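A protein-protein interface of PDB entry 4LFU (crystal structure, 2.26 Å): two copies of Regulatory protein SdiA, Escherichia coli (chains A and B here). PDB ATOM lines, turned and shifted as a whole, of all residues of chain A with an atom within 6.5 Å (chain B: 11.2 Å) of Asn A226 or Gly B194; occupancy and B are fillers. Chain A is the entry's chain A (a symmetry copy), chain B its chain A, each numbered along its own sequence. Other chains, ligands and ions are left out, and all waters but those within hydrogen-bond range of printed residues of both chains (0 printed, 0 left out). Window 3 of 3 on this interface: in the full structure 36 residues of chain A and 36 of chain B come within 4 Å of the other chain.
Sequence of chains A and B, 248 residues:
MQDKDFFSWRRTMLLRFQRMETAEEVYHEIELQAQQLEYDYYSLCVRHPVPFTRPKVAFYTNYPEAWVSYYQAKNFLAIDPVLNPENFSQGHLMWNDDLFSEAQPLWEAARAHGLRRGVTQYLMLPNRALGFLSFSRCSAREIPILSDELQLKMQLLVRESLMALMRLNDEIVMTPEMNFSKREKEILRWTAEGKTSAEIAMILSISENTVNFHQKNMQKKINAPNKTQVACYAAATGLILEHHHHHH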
ATOM      1  N   GLN A 215     -16.216 -15.614  17.448  1.00  0.00           N
ATOM      2  CA  GLN A 215     -15.664 -14.861  18.579  1.00  0.00           C
ATOM      3  C   GLN A 215     -14.674 -15.701  19.368  1.00  0.00           C
ATOM      4  O   GLN A 215     -13.561 -15.263  19.635  1.00  0.00           O
ATOM      5  CB  GLN A 215     -16.757 -14.344  19.540  1.00  0.00           C
ATOM      6  CG  GLN A 215     -17.756 -13.337  18.980  1.00  0.00           C
ATOM      7  CD  GLN A 215     -17.177 -11.957  18.703  1.00  0.00           C
ATOM      8  OE1 GLN A 215     -15.957 -11.754  18.667  1.00  0.00           O
ATOM      9  NE2 GLN A 215     -18.071 -10.998  18.456  1.00  0.00           N
ATOM     10  N   LYS A 216     -15.112 -16.903  19.720  1.00  0.00           N
ATOM     11  CA  LYS A 216     -14.317 -17.916  20.404  1.00  0.00           C
ATOM     12  C   LYS A 216     -13.035 -18.317  19.712  1.00  0.00           C
ATOM     13  O   LYS A 216     -12.012 -18.460  20.377  1.00  0.00           O
ATOM     14  CB  LYS A 216     -15.166 -19.164  20.648  1.00  0.00           C
ATOM     15  CG  LYS A 216     -15.664 -19.298  22.082  1.00  0.00           C
ATOM     16  CD  LYS A 216     -16.325 -18.003  22.600  1.00  0.00           C
ATOM     17  CE  LYS A 216     -15.905 -17.684  24.031  1.00  0.00           C
ATOM     18  NZ  LYS A 216     -16.445 -16.345  24.467  1.00  0.00           N
ATOM     19  N   GLN A 219     -10.583 -15.459  19.946  1.00  0.00           N
ATOM     20  CA  GLN A 219     -10.127 -15.433  21.334  1.00  0.00           C
ATOM     21  C   GLN A 219      -9.083 -16.499  21.539  1.00  0.00           C
ATOM     22  O   GLN A 219      -8.020 -16.220  22.083  1.00  0.00           O
ATOM     23  CB  GLN A 219     -11.304 -15.617  22.311  1.00  0.00           C
ATOM     24  CG  GLN A 219     -11.992 -14.316  22.631  1.00  0.00           C
ATOM     25  CD  GLN A 219     -13.420 -14.456  23.103  1.00  0.00           C
ATOM     26  OE1 GLN A 219     -14.332 -13.833  22.539  1.00  0.00           O
ATOM     27  NE2 GLN A 219     -13.632 -15.237  24.150  1.00  0.00           N
ATOM     28  N   ALA A 224      -6.948 -14.281  24.073  1.00  0.00           N
ATOM     29  CA  ALA A 224      -7.688 -13.180  24.688  1.00  0.00           C
ATOM     30  C   ALA A 224      -8.760 -13.676  25.661  1.00  0.00           C
ATOM     31  O   ALA A 224      -9.325 -14.729  25.442  1.00  0.00           O
ATOM     32  CB  ALA A 224      -8.320 -12.299  23.612  1.00  0.00           C
ATOM     33  N   PRO A 225      -9.022 -12.925  26.762  1.00  0.00           N
ATOM     34  CA  PRO A 225     -10.126 -13.311  27.674  1.00  0.00           C
ATOM     35  C   PRO A 225     -11.567 -13.002  27.183  1.00  0.00           C
ATOM     36  O   PRO A 225     -12.532 -13.575  27.702  1.00  0.00           O
ATOM     37  CB  PRO A 225      -9.817 -12.512  28.949  1.00  0.00           C
ATOM     38  CG  PRO A 225      -9.094 -11.323  28.477  1.00  0.00           C
ATOM     39  CD  PRO A 225      -8.295 -11.734  27.256  1.00  0.00           C
ATOM     40  N   ASN A 226     -11.714 -12.097  26.221  1.00  0.00           N
ATOM     41  CA  ASN A 226     -13.039 -11.714  25.715  1.00  0.00           C
ATOM     42  C   ASN A 226     -12.924 -11.002  24.358  1.00  0.00           C
ATOM     43  O   ASN A 226     -11.830 -10.770  23.887  1.00  0.00           O
ATOM     44  CB  ASN A 226     -13.789 -10.825  26.732  1.00  0.00           C
ATOM     45  CG  ASN A 226     -12.933  -9.690  27.267  1.00  0.00           C
ATOM     46  OD1 ASN A 226     -12.769  -9.565  28.471  1.00  0.00           O
ATOM     47  ND2 ASN A 226     -12.349  -8.896  26.388  1.00  0.00           N
ATOM     48  N   LYS A 227     -14.065 -10.653  23.762  1.00  0.00           N
ATOM     49  CA  LYS A 227     -14.142 -10.023  22.441  1.00  0.00           C
ATOM     50  C   LYS A 227     -13.631  -8.568  22.415  1.00  0.00           C
ATOM     51  O   LYS A 227     -13.189  -8.080  21.374  1.00  0.00           O
ATOM     52  CB  LYS A 227     -15.591 -10.073  21.936  1.00  0.00           C
ATOM     53  CG  LYS A 227     -16.591  -9.259  22.760  1.00  0.00           C
ATOM     54  CD  LYS A 227     -18.030  -9.656  22.467  1.00  0.00           C
ATOM     55  CE  LYS A 227     -18.980  -8.505  22.787  1.00  0.00           C
ATOM     56  NZ  LYS A 227     -20.403  -8.848  22.517  1.00  0.00           N
ATOM     57  N   THR A 228     -13.724  -7.886  23.560  1.00  0.00           N
ATOM     58  CA  THR A 228     -13.299  -6.476  23.695  1.00  0.00           C
ATOM     59  C   THR A 228     -11.825  -6.324  23.445  1.00  0.00           C
ATOM     60  O   THR A 228     -11.433  -5.434  22.692  1.00  0.00           O
ATOM     61  CB  THR A 228     -13.641  -5.849  25.083  1.00  0.00           C
ATOM     62  OG1 THR A 228     -15.014  -6.105  25.406  1.00  0.00           O
ATOM     63  CG2 THR A 228     -13.397  -4.323  25.059  1.00  0.00           C
ATOM     64  N   GLN A 229     -11.027  -7.189  24.075  1.00  0.00           N
ATOM     65  CA  GLN A 229      -9.573  -7.212  23.869  1.00  0.00           C
ATOM     66  C   GLN A 229      -9.228  -7.547  22.413  1.00  0.00           C
ATOM     67  O   GLN A 229      -8.313  -6.956  21.832  1.00  0.00           O
ATOM     68  CB  GLN A 229      -8.835  -8.187  24.832  1.00  0.00           C
ATOM     69  CG  GLN A 229      -7.309  -8.107  24.578  1.00  0.00           C
ATOM     70  CD  GLN A 229      -6.464  -9.163  25.262  1.00  0.00           C
ATOM     71  OE1 GLN A 229      -6.186  -9.070  26.450  1.00  0.00           O
ATOM     72  NE2 GLN A 229      -5.990 -10.143  24.489  1.00  0.00           N
ATOM     73  N   VAL A 230      -9.964  -8.489  21.817  1.00  0.00           N
ATOM     74  CA  VAL A 230      -9.732  -8.830  20.392  1.00  0.00           C
ATOM     75  C   VAL A 230     -10.023  -7.654  19.472  1.00  0.00           C
ATOM     76  O   VAL A 230      -9.190  -7.281  18.634  1.00  0.00           O
ATOM     77  CB  VAL A 230     -10.555 -10.035  19.927  1.00  0.00           C
ATOM     78  CG1 VAL A 230     -10.205 -10.368  18.470  1.00  0.00           C
ATOM     79  CG2 VAL A 230     -10.298 -11.197  20.817  1.00  0.00           C
ATOM     80  N   ALA A 231     -11.196  -7.057  19.640  1.00  0.00           N
ATOM     81  CA  ALA A 231     -11.578  -5.904  18.843  1.00  0.00           C
ATOM     82  C   ALA A 231     -10.630  -4.713  19.043  1.00  0.00           C
ATOM     83  O   ALA A 231     -10.261  -4.041  18.079  1.00  0.00           O
ATOM     84  CB  ALA A 231     -13.031  -5.510  19.149  1.00  0.00           C
ATOM     85  N   TYR A 233      -7.408  -4.707  20.148  1.00  0.00           N
ATOM     86  CA  TYR A 233      -6.110  -5.036  19.552  1.00  0.00           C
ATOM     87  C   TYR A 233      -6.118  -4.902  18.022  1.00  0.00           C
ATOM     88  O   TYR A 233      -5.212  -4.287  17.429  1.00  0.00           O
ATOM     89  CB  TYR A 233      -5.656  -6.431  19.991  1.00  0.00           C
ATOM     90  CG  TYR A 233      -4.874  -6.444  21.295  1.00  0.00           C
ATOM     91  CD1 TYR A 233      -5.407  -5.907  22.459  1.00  0.00           C
ATOM     92  CD2 TYR A 233      -3.592  -7.000  21.356  1.00  0.00           C
ATOM     93  CE1 TYR A 233      -4.694  -5.933  23.658  1.00  0.00           C
ATOM     94  CE2 TYR A 233      -2.858  -7.024  22.562  1.00  0.00           C
ATOM     95  CZ  TYR A 233      -3.421  -6.491  23.701  1.00  0.00           C
ATOM     96  OH  TYR A 233      -2.718  -6.524  24.883  1.00  0.00           O
ATOM     97  N   GLU B 186      -7.591   6.146  31.611  1.00  0.00           N
ATOM     98  CA  GLU B 186      -6.982   5.048  32.380  1.00  0.00           C
ATOM     99  C   GLU B 186      -7.891   3.817  32.484  1.00  0.00           C
ATOM    100  O   GLU B 186      -7.461   2.703  32.224  1.00  0.00           O
ATOM    101  CB  GLU B 186      -6.546   5.538  33.766  1.00  0.00           C
ATOM    102  CG  GLU B 186      -6.086   4.427  34.722  1.00  0.00           C
ATOM    103  CD  GLU B 186      -5.577   4.985  36.046  1.00  0.00           C
ATOM    104  OE1 GLU B 186      -6.303   5.790  36.664  1.00  0.00           O
ATOM    105  OE2 GLU B 186      -4.443   4.637  36.465  1.00  0.00           O
ATOM    106  N   ILE B 187      -9.139   4.023  32.890  1.00  0.00           N
ATOM    107  CA  ILE B 187     -10.167   2.976  32.855  1.00  0.00           C
ATOM    108  C   ILE B 187     -10.389   2.374  31.446  1.00  0.00           C
ATOM    109  O   ILE B 187     -10.559   1.174  31.305  1.00  0.00           O
ATOM    110  CB  ILE B 187     -11.500   3.478  33.497  1.00  0.00           C
ATOM    111  CG1 ILE B 187     -11.355   3.507  35.036  1.00  0.00           C
ATOM    112  CG2 ILE B 187     -12.724   2.580  33.086  1.00  0.00           C
ATOM    113  CD1 ILE B 187     -12.292   4.449  35.740  1.00  0.00           C
ATOM    114  N   LEU B 188     -10.361   3.219  30.413  1.00  0.00           N
ATOM    115  CA  LEU B 188     -10.513   2.769  29.034  1.00  0.00           C
ATOM    116  C   LEU B 188      -9.415   1.800  28.629  1.00  0.00           C
ATOM    117  O   LEU B 188      -9.694   0.745  28.075  1.00  0.00           O
ATOM    118  CB  LEU B 188     -10.575   3.960  28.089  1.00  0.00           C
ATOM    119  CG  LEU B 188     -11.473   3.689  26.882  1.00  0.00           C
ATOM    120  CD1 LEU B 188     -12.893   3.215  27.309  1.00  0.00           C
ATOM    121  CD2 LEU B 188     -11.505   4.944  26.029  1.00  0.00           C
ATOM    122  N   ARG B 189      -8.175   2.147  28.956  1.00  0.00           N
ATOM    123  CA  ARG B 189      -7.013   1.272  28.730  1.00  0.00           C
ATOM    124  C   ARG B 189      -7.114  -0.122  29.323  1.00  0.00           C
ATOM    125  O   ARG B 189      -6.720  -1.101  28.676  1.00  0.00           O
ATOM    126  CB  ARG B 189      -5.723   1.950  29.197  1.00  0.00           C
ATOM    127  CG  ARG B 189      -5.302   3.109  28.290  1.00  0.00           C
ATOM    128  CD  ARG B 189      -3.840   3.522  28.558  1.00  0.00           C
ATOM    129  NE  ARG B 189      -3.676   4.075  29.909  1.00  0.00           N
ATOM    130  CZ  ARG B 189      -3.945   5.336  30.241  1.00  0.00           C
ATOM    131  NH1 ARG B 189      -4.386   6.205  29.327  1.00  0.00           N
ATOM    132  NH2 ARG B 189      -3.755   5.731  31.487  1.00  0.00           N
ATOM    133  N   TRP B 190      -7.625  -0.223  30.548  1.00  0.00           N
ATOM    134  CA  TRP B 190      -7.822  -1.528  31.189  1.00  0.00           C
ATOM    135  C   TRP B 190      -8.971  -2.286  30.531  1.00  0.00           C
ATOM    136  O   TRP B 190      -8.949  -3.525  30.471  1.00  0.00           O
ATOM    137  CB  TRP B 190      -8.023  -1.410  32.730  1.00  0.00           C
ATOM    138  CG  TRP B 190      -6.759  -1.061  33.445  1.00  0.00           C
ATOM    139  CD1 TRP B 190      -6.436   0.153  33.975  1.00  0.00           C
ATOM    140  CD2 TRP B 190      -5.616  -1.912  33.665  1.00  0.00           C
ATOM    141  NE1 TRP B 190      -5.173   0.116  34.519  1.00  0.00           N
ATOM    142  CE2 TRP B 190      -4.645  -1.135  34.342  1.00  0.00           C
ATOM    143  CE3 TRP B 190      -5.321  -3.254  33.360  1.00  0.00           C
ATOM    144  CZ2 TRP B 190      -3.399  -1.653  34.724  1.00  0.00           C
ATOM    145  CZ3 TRP B 190      -4.081  -3.774  33.738  1.00  0.00           C
ATOM    146  CH2 TRP B 190      -3.132  -2.974  34.411  1.00  0.00           C
ATOM    147  N   THR B 191      -9.963  -1.535  30.051  1.00  0.00           N
ATOM    148  CA  THR B 191     -11.085  -2.101  29.284  1.00  0.00           C
ATOM    149  C   THR B 191     -10.611  -2.781  27.975  1.00  0.00           C
ATOM    150  O   THR B 191     -10.977  -3.934  27.667  1.00  0.00           O
ATOM    151  CB  THR B 191     -12.159  -1.017  29.028  1.00  0.00           C
ATOM    152  OG1 THR B 191     -12.656  -0.582  30.294  1.00  0.00           O
ATOM    153  CG2 THR B 191     -13.340  -1.555  28.168  1.00  0.00           C
ATOM    154  N   ALA B 192      -9.763  -2.064  27.248  1.00  0.00           N
ATOM    155  CA  ALA B 192      -9.193  -2.527  25.996  1.00  0.00           C
ATOM    156  C   ALA B 192      -8.277  -3.738  26.175  1.00  0.00           C
ATOM    157  O   ALA B 192      -8.014  -4.453  25.211  1.00  0.00           O
ATOM    158  CB  ALA B 192      -8.452  -1.373  25.321  1.00  0.00           C
ATOM    159  N   GLU B 193      -7.797  -3.959  27.407  1.00  0.00           N
ATOM    160  CA  GLU B 193      -6.931  -5.093  27.741  1.00  0.00           C
ATOM    161  C   GLU B 193      -7.727  -6.317  28.152  1.00  0.00           C
ATOM    162  O   GLU B 193      -7.149  -7.373  28.417  1.00  0.00           O
ATOM    163  CB  GLU B 193      -5.947  -4.751  28.867  1.00  0.00           C
ATOM    164  CG  GLU B 193      -4.762  -3.880  28.454  1.00  0.00           C
ATOM    165  CD  GLU B 193      -3.865  -4.517  27.396  1.00  0.00           C
ATOM    166  OE1 GLU B 193      -3.878  -5.748  27.171  1.00  0.00           O
ATOM    167  OE2 GLU B 193      -3.131  -3.761  26.754  1.00  0.00           O
ATOM    168  N   GLY B 194      -9.047  -6.169  28.220  1.00  0.00           N
ATOM    169  CA  GLY B 194      -9.935  -7.276  28.549  1.00  0.00           C
ATOM    170  C   GLY B 194     -10.334  -7.378  30.009  1.00  0.00           C
ATOM    171  O   GLY B 194     -10.924  -8.382  30.412  1.00  0.00           O
ATOM    172  N   LYS B 195     -10.059  -6.339  30.801  1.00  0.00           N
ATOM    173  CA  LYS B 195     -10.442  -6.378  32.207  1.00  0.00           C
ATOM    174  C   LYS B 195     -11.920  -6.080  32.389  1.00  0.00           C
ATOM    175  O   LYS B 195     -12.491  -5.241  31.685  1.00  0.00           O
ATOM    176  CB  LYS B 195      -9.581  -5.444  33.059  1.00  0.00           C
ATOM    177  CG  LYS B 195      -8.081  -5.679  32.958  1.00  0.00           C
ATOM    178  CD  LYS B 195      -7.667  -7.043  33.513  1.00  0.00           C
ATOM    179  CE  LYS B 195      -6.158  -7.242  33.443  1.00  0.00           C
ATOM    180  NZ  LYS B 195      -5.798  -8.662  33.764  1.00  0.00           N
ATOM    181  N   THR B 196     -12.538  -6.804  33.319  1.00  0.00           N
ATOM    182  CA  THR B 196     -13.908  -6.538  33.774  1.00  0.00           C
ATOM    183  C   THR B 196     -13.966  -5.316  34.751  1.00  0.00           C
ATOM    184  O   THR B 196     -12.937  -4.864  35.269  1.00  0.00           O
ATOM    185  CB  THR B 196     -14.492  -7.801  34.450  1.00  0.00           C
ATOM    186  OG1 THR B 196     -13.703  -8.129  35.604  1.00  0.00           O
ATOM    187  CG2 THR B 196     -14.474  -8.985  33.487  1.00  0.00           C
ATOM    188  N   SER B 197     -15.161  -4.782  34.980  1.00  0.00           N
ATOM    189  CA  SER B 197     -15.362  -3.748  35.999  1.00  0.00           C
ATOM    190  C   SER B 197     -14.773  -4.116  37.364  1.00  0.00           C
ATOM    191  O   SER B 197     -14.166  -3.264  38.017  1.00  0.00           O
ATOM    192  CB  SER B 197     -16.843  -3.421  36.175  1.00  0.00           C
ATOM    193  OG  SER B 197     -17.239  -2.510  35.171  1.00  0.00           O
ATOM    194  N   ALA B 198     -14.948  -5.379  37.770  1.00  0.00           N
ATOM    195  CA  ALA B 198     -14.448  -5.892  39.059  1.00  0.00           C
ATOM    196  C   ALA B 198     -12.926  -5.907  39.146  1.00  0.00           C
ATOM    197  O   ALA B 198     -12.348  -5.532  40.175  1.00  0.00           O
ATOM    198  CB  ALA B 198     -15.005  -7.281  39.324  1.00  0.00           C
ATOM    199  N   GLU B 199     -12.290  -6.347  38.065  1.00  0.00           N
ATOM    200  CA  GLU B 199     -10.839  -6.390  37.972  1.00  0.00           C
ATOM    201  C   GLU B 199     -10.229  -4.993  37.931  1.00  0.00           C
ATOM    202  O   GLU B 199      -9.200  -4.744  38.556  1.00  0.00           O
ATOM    203  CB  GLU B 199     -10.401  -7.188  36.746  1.00  0.00           C
ATOM    204  CG  GLU B 199     -10.516  -8.696  36.911  1.00  0.00           C
ATOM    205  CD  GLU B 199     -10.319  -9.460  35.586  1.00  0.00           C
ATOM    206  OE1 GLU B 199     -10.930  -9.091  34.553  1.00  0.00           O
ATOM    207  OE2 GLU B 199      -9.553 -10.455  35.587  1.00  0.00           O
ATOM    208  N   ILE B 200     -10.860  -4.091  37.184  1.00  0.00           N
ATOM    209  CA  ILE B 200     -10.422  -2.701  37.143  1.00  0.00           C
ATOM    210  C   ILE B 200     -10.546  -2.034  38.533  1.00  0.00           C
ATOM    211  O   ILE B 200      -9.683  -1.260  38.928  1.00  0.00           O
ATOM    212  CB  ILE B 200     -11.161  -1.891  36.014  1.00  0.00           C
ATOM    213  CG1 ILE B 200     -10.855  -2.524  34.642  1.00  0.00           C
ATOM    214  CG2 ILE B 200     -10.745  -0.417  36.017  1.00  0.00           C
ATOM    215  CD1 ILE B 200     -11.704  -2.014  33.475  1.00  0.00           C
ATOM    216  N   ALA B 201     -11.613  -2.357  39.263  1.00  0.00           N
ATOM    217  CA  ALA B 201     -11.832  -1.851  40.624  1.00  0.00           C
ATOM    218  C   ALA B 201     -10.681  -2.258  41.564  1.00  0.00           C
ATOM    219  O   ALA B 201     -10.192  -1.436  42.339  1.00  0.00           O
ATOM    220  CB  ALA B 201     -13.179  -2.332  41.166  1.00  0.00           C
ATOM    221  N   ILE B 203      -7.513  -3.318  40.489  1.00  0.00           N
ATOM    222  CA  ILE B 203      -6.314  -2.656  39.938  1.00  0.00           C
ATOM    223  C   ILE B 203      -6.142  -1.237  40.465  1.00  0.00           C
ATOM    224  O   ILE B 203      -5.045  -0.837  40.849  1.00  0.00           O
ATOM    225  CB  ILE B 203      -6.340  -2.560  38.373  1.00  0.00           C
ATOM    226  CG1 ILE B 203      -6.709  -3.901  37.716  1.00  0.00           C
ATOM    227  CG2 ILE B 203      -5.028  -1.920  37.825  1.00  0.00           C
ATOM    228  CD1 ILE B 203      -5.589  -4.866  37.525  1.00  0.00           C
ATOM    229  N   VAL B 211     -15.974   2.793  38.633  1.00  0.00           N
ATOM    230  CA  VAL B 211     -15.576   2.324  37.317  1.00  0.00           C
ATOM    231  C   VAL B 211     -16.733   2.557  36.345  1.00  0.00           C
ATOM    232  O   VAL B 211     -16.550   3.204  35.326  1.00  0.00           O
ATOM    233  CB  VAL B 211     -15.123   0.809  37.303  1.00  0.00           C
ATOM    234  CG1 VAL B 211     -14.928   0.329  35.871  1.00  0.00           C
ATOM    235  CG2 VAL B 211     -13.820   0.600  38.104  1.00  0.00           C
ATOM    236  N   GLN B 215     -17.332   4.825  32.885  1.00  0.00           N
ATOM    237  CA  GLN B 215     -17.765   4.153  31.655  1.00  0.00           C
ATOM    238  C   GLN B 215     -18.974   4.844  31.047  1.00  0.00           C
ATOM    239  O   GLN B 215     -18.979   5.160  29.863  1.00  0.00           O
ATOM    240  CB  GLN B 215     -18.104   2.663  31.880  1.00  0.00           C
ATOM    241  CG  GLN B 215     -16.965   1.751  32.324  1.00  0.00           C
ATOM    242  CD  GLN B 215     -15.918   1.476  31.255  1.00  0.00           C
ATOM    243  OE1 GLN B 215     -15.846   2.152  30.221  1.00  0.00           O
ATOM    244  NE2 GLN B 215     -15.059   0.494  31.530  1.00  0.00           N
ATOM    245  N   LYS B 227     -19.208   0.052  26.343  1.00  0.00           N
ATOM    246  CA  LYS B 227     -17.785   0.337  26.549  1.00  0.00           C
ATOM    247  C   LYS B 227     -16.879  -0.154  25.401  1.00  0.00           C
ATOM    248  O   LYS B 227     -15.798   0.393  25.181  1.00  0.00           O
ATOM    249  CB  LYS B 227     -17.327  -0.287  27.875  1.00  0.00           C
ATOM    250  CG  LYS B 227     -17.378  -1.816  27.921  1.00  0.00           C
ATOM    251  CD  LYS B 227     -17.304  -2.347  29.345  1.00  0.00           C
ATOM    252  CE  LYS B 227     -16.757  -3.772  29.358  1.00  0.00           C
ATOM    253  NZ  LYS B 227     -16.668  -4.335  30.733  1.00  0.00           N
ATOM    254  N   THR B 228     -17.323  -1.202  24.702  1.00  0.00           N
ATOM    255  CA  THR B 228     -16.565  -1.807  23.586  1.00  0.00           C
ATOM    256  C   THR B 228     -16.377  -0.829  22.461  1.00  0.00           C
ATOM    257  O   THR B 228     -15.259  -0.693  21.964  1.00  0.00           O
ATOM    258  CB  THR B 228     -17.214  -3.108  23.019  1.00  0.00           C
ATOM    259  OG1 THR B 228     -17.530  -4.001  24.096  1.00  0.00           O
ATOM    260  CG2 THR B 228     -16.246  -3.810  22.040  1.00  0.00           C
ATOM    261  N   GLN B 229     -17.465  -0.162  22.071  1.00  0.00           N
ATOM    262  CA  GLN B 229     -17.421   0.880  21.037  1.00  0.00           C
ATOM    263  C   GLN B 229     -16.535   2.053  21.473  1.00  0.00           C
ATOM    264  O   GLN B 229     -15.776   2.600  20.667  1.00  0.00           O
ATOM    265  CB  GLN B 229     -18.832   1.398  20.630  1.00  0.00           C
ATOM    266  CG  GLN B 229     -18.691   2.451  19.503  1.00  0.00           C
ATOM    267  CD  GLN B 229     -19.945   3.229  19.158  1.00  0.00           C
ATOM    268  OE1 GLN B 229     -20.821   2.730  18.466  1.00  0.00           O
ATOM    269  NE2 GLN B 229     -20.002   4.492  19.587  1.00  0.00           N
ATOM    270  N   ALA B 231     -13.951   1.982  23.735  1.00  0.00           N
ATOM    271  CA  ALA B 231     -12.580   1.501  23.713  1.00  0.00           C
ATOM    272  C   ALA B 231     -12.046   1.319  22.286  1.00  0.00           C
ATOM    273  O   ALA B 231     -10.902   1.674  21.998  1.00  0.00           O
ATOM    274  CB  ALA B 231     -12.467   0.196  24.517  1.00  0.00           C
ATOM    275  N   CYS B 232     -12.862   0.761  21.389  1.00  0.00           N
ATOM    276  CA  CYS B 232     -12.422   0.532  19.991  1.00  0.00           C
ATOM    277  C   CYS B 232     -12.223   1.806  19.217  1.00  0.00           C
ATOM    278  O   CYS B 232     -11.285   1.906  18.470  1.00  0.00           O
ATOM    279  CB  CYS B 232     -13.402  -0.361  19.241  1.00  0.00           C
ATOM    280  SG  CYS B 232     -13.317  -2.027  19.822  1.00  0.00           S
ATOM    281  N   ALA B 235      -9.021   3.278  20.700  1.00  0.00           N
ATOM    282  CA  ALA B 235      -7.922   2.476  20.199  1.00  0.00           C
ATOM    283  C   ALA B 235      -7.627   2.805  18.718  1.00  0.00           C
ATOM    284  O   ALA B 235      -6.454   2.992  18.349  1.00  0.00           O
ATOM    285  CB  ALA B 235      -8.229   1.035  20.373  1.00  0.00           C
ATOM    286  N   ILE B 240      -6.388   6.493  23.137  1.00  0.00           N
ATOM    287  CA  ILE B 240      -5.866   5.541  24.113  1.00  0.00           C
ATOM    288  C   ILE B 240      -4.321   5.486  24.093  1.00  0.00           C
ATOM    289  O   ILE B 240      -3.647   5.828  23.103  1.00  0.00           O
ATOM    290  CB  ILE B 240      -6.469   4.122  23.780  1.00  0.00           C
ATOM    291  CG1 ILE B 240      -7.528   3.695  24.801  1.00  0.00           C
ATOM    292  CG2 ILE B 240      -5.394   3.074  23.665  1.00  0.00           C
ATOM    293  CD1 ILE B 240      -8.068   2.287  24.565  1.00  0.00           C
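Thr A228 touches its own counterpart, Thr B228. Positions printed for both chains: 215, 227, 228, 229 and 231.
Pro A225 touches Gly B194 (CG to O, 3.97 Å). CG2 of Thr A228 touches O of Thr B191 (3.6 Å). OG1 of Thr A228 touches OG1 of Thr B228, at 3.5 Å. Ala B192 touches Gln A229 (O to CA, 3.4 Å). Gly B194 touches Gln A229. Ala A231 touches Cys B232 (CB to SG, 3.6 Å). Tyr A233 touches Ala B192 (CE1 to O, 3.95 Å).
Hydrophobic or aromatic side chains of chain A that line the printed part of chain B: Pro A225, Ala A231 and Tyr A233. Along chain A the printed residues that touch a printed residue of chain B span positions 225 to 233. Of the 26 printed residues of chain B, 6 touch a printed residue of chain A. Among the printed residues, 10 pairs touch across the chains. Among the printed residues, no Asp or Glu carboxylate lies within 4 Å of a Lys or Arg side-chain nitrogen of the other chain.
OE1 of Glu B193 sits at hydrogen-bond distance from OH of Tyr A233 (2.7 Å). The backbone carbonyl oxygen (O) of Glu B193 lies close to the side-chain amide oxygen (OE1) of Gln A229 (2.8 Å). The side-chain amide oxygen (OD1) of Asn A226 sits close to the backbone carbonyl oxygen (O) of Gly B194 (2.9 Å).
No residue of chain B comes within 4 Å of Gln A219. Printed residues of chain B within 4 Å of Pro A225: Gly B194 (3.97 Å). Of the printed residues of chain B, Asn A226 touches Gly B194 (2.9 Å). Gln A229 touches just these residues of chain B: Ala B192, Glu B193 and Gly B194. Val A230 touches none of the printed residues of chain B. Of the printed residues of chain B, Tyr A233 touches Ala B192 and Glu B193. Printed residues of chain A within 4 Å of Ala B192: Gln A229 (3.4 Å) and Tyr A233 (3.95 Å). Of the printed residues of chain A, Glu B193 touches Gln A229 and Tyr A233. Gln B229 touches none of the printed residues of chain A. Of the printed residues of chain A, Cys B232 touches Ala A231. The nearest printed residue of chain B that does not touch Ala A231 is Thr B228 (4.6 Å).
The side-chain hydroxyl of Thr B191 sits at hydrogen-bond distance from the side-chain amide nitrogen of Gln B215. O of Thr B228 is in hydrogen-bond range of SG of Cys B232 (3.2 Å). O of Ile B187 sits at hydrogen-bond distance from OG1 of Thr B191. The backbone NH (N) of Thr A228 lies close to the side-chain amide nitrogen (ND2) of Asn A226 (3.3 Å). ND2 of Asn A226 sits close to N of Gln A229, 3.2 Å away.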
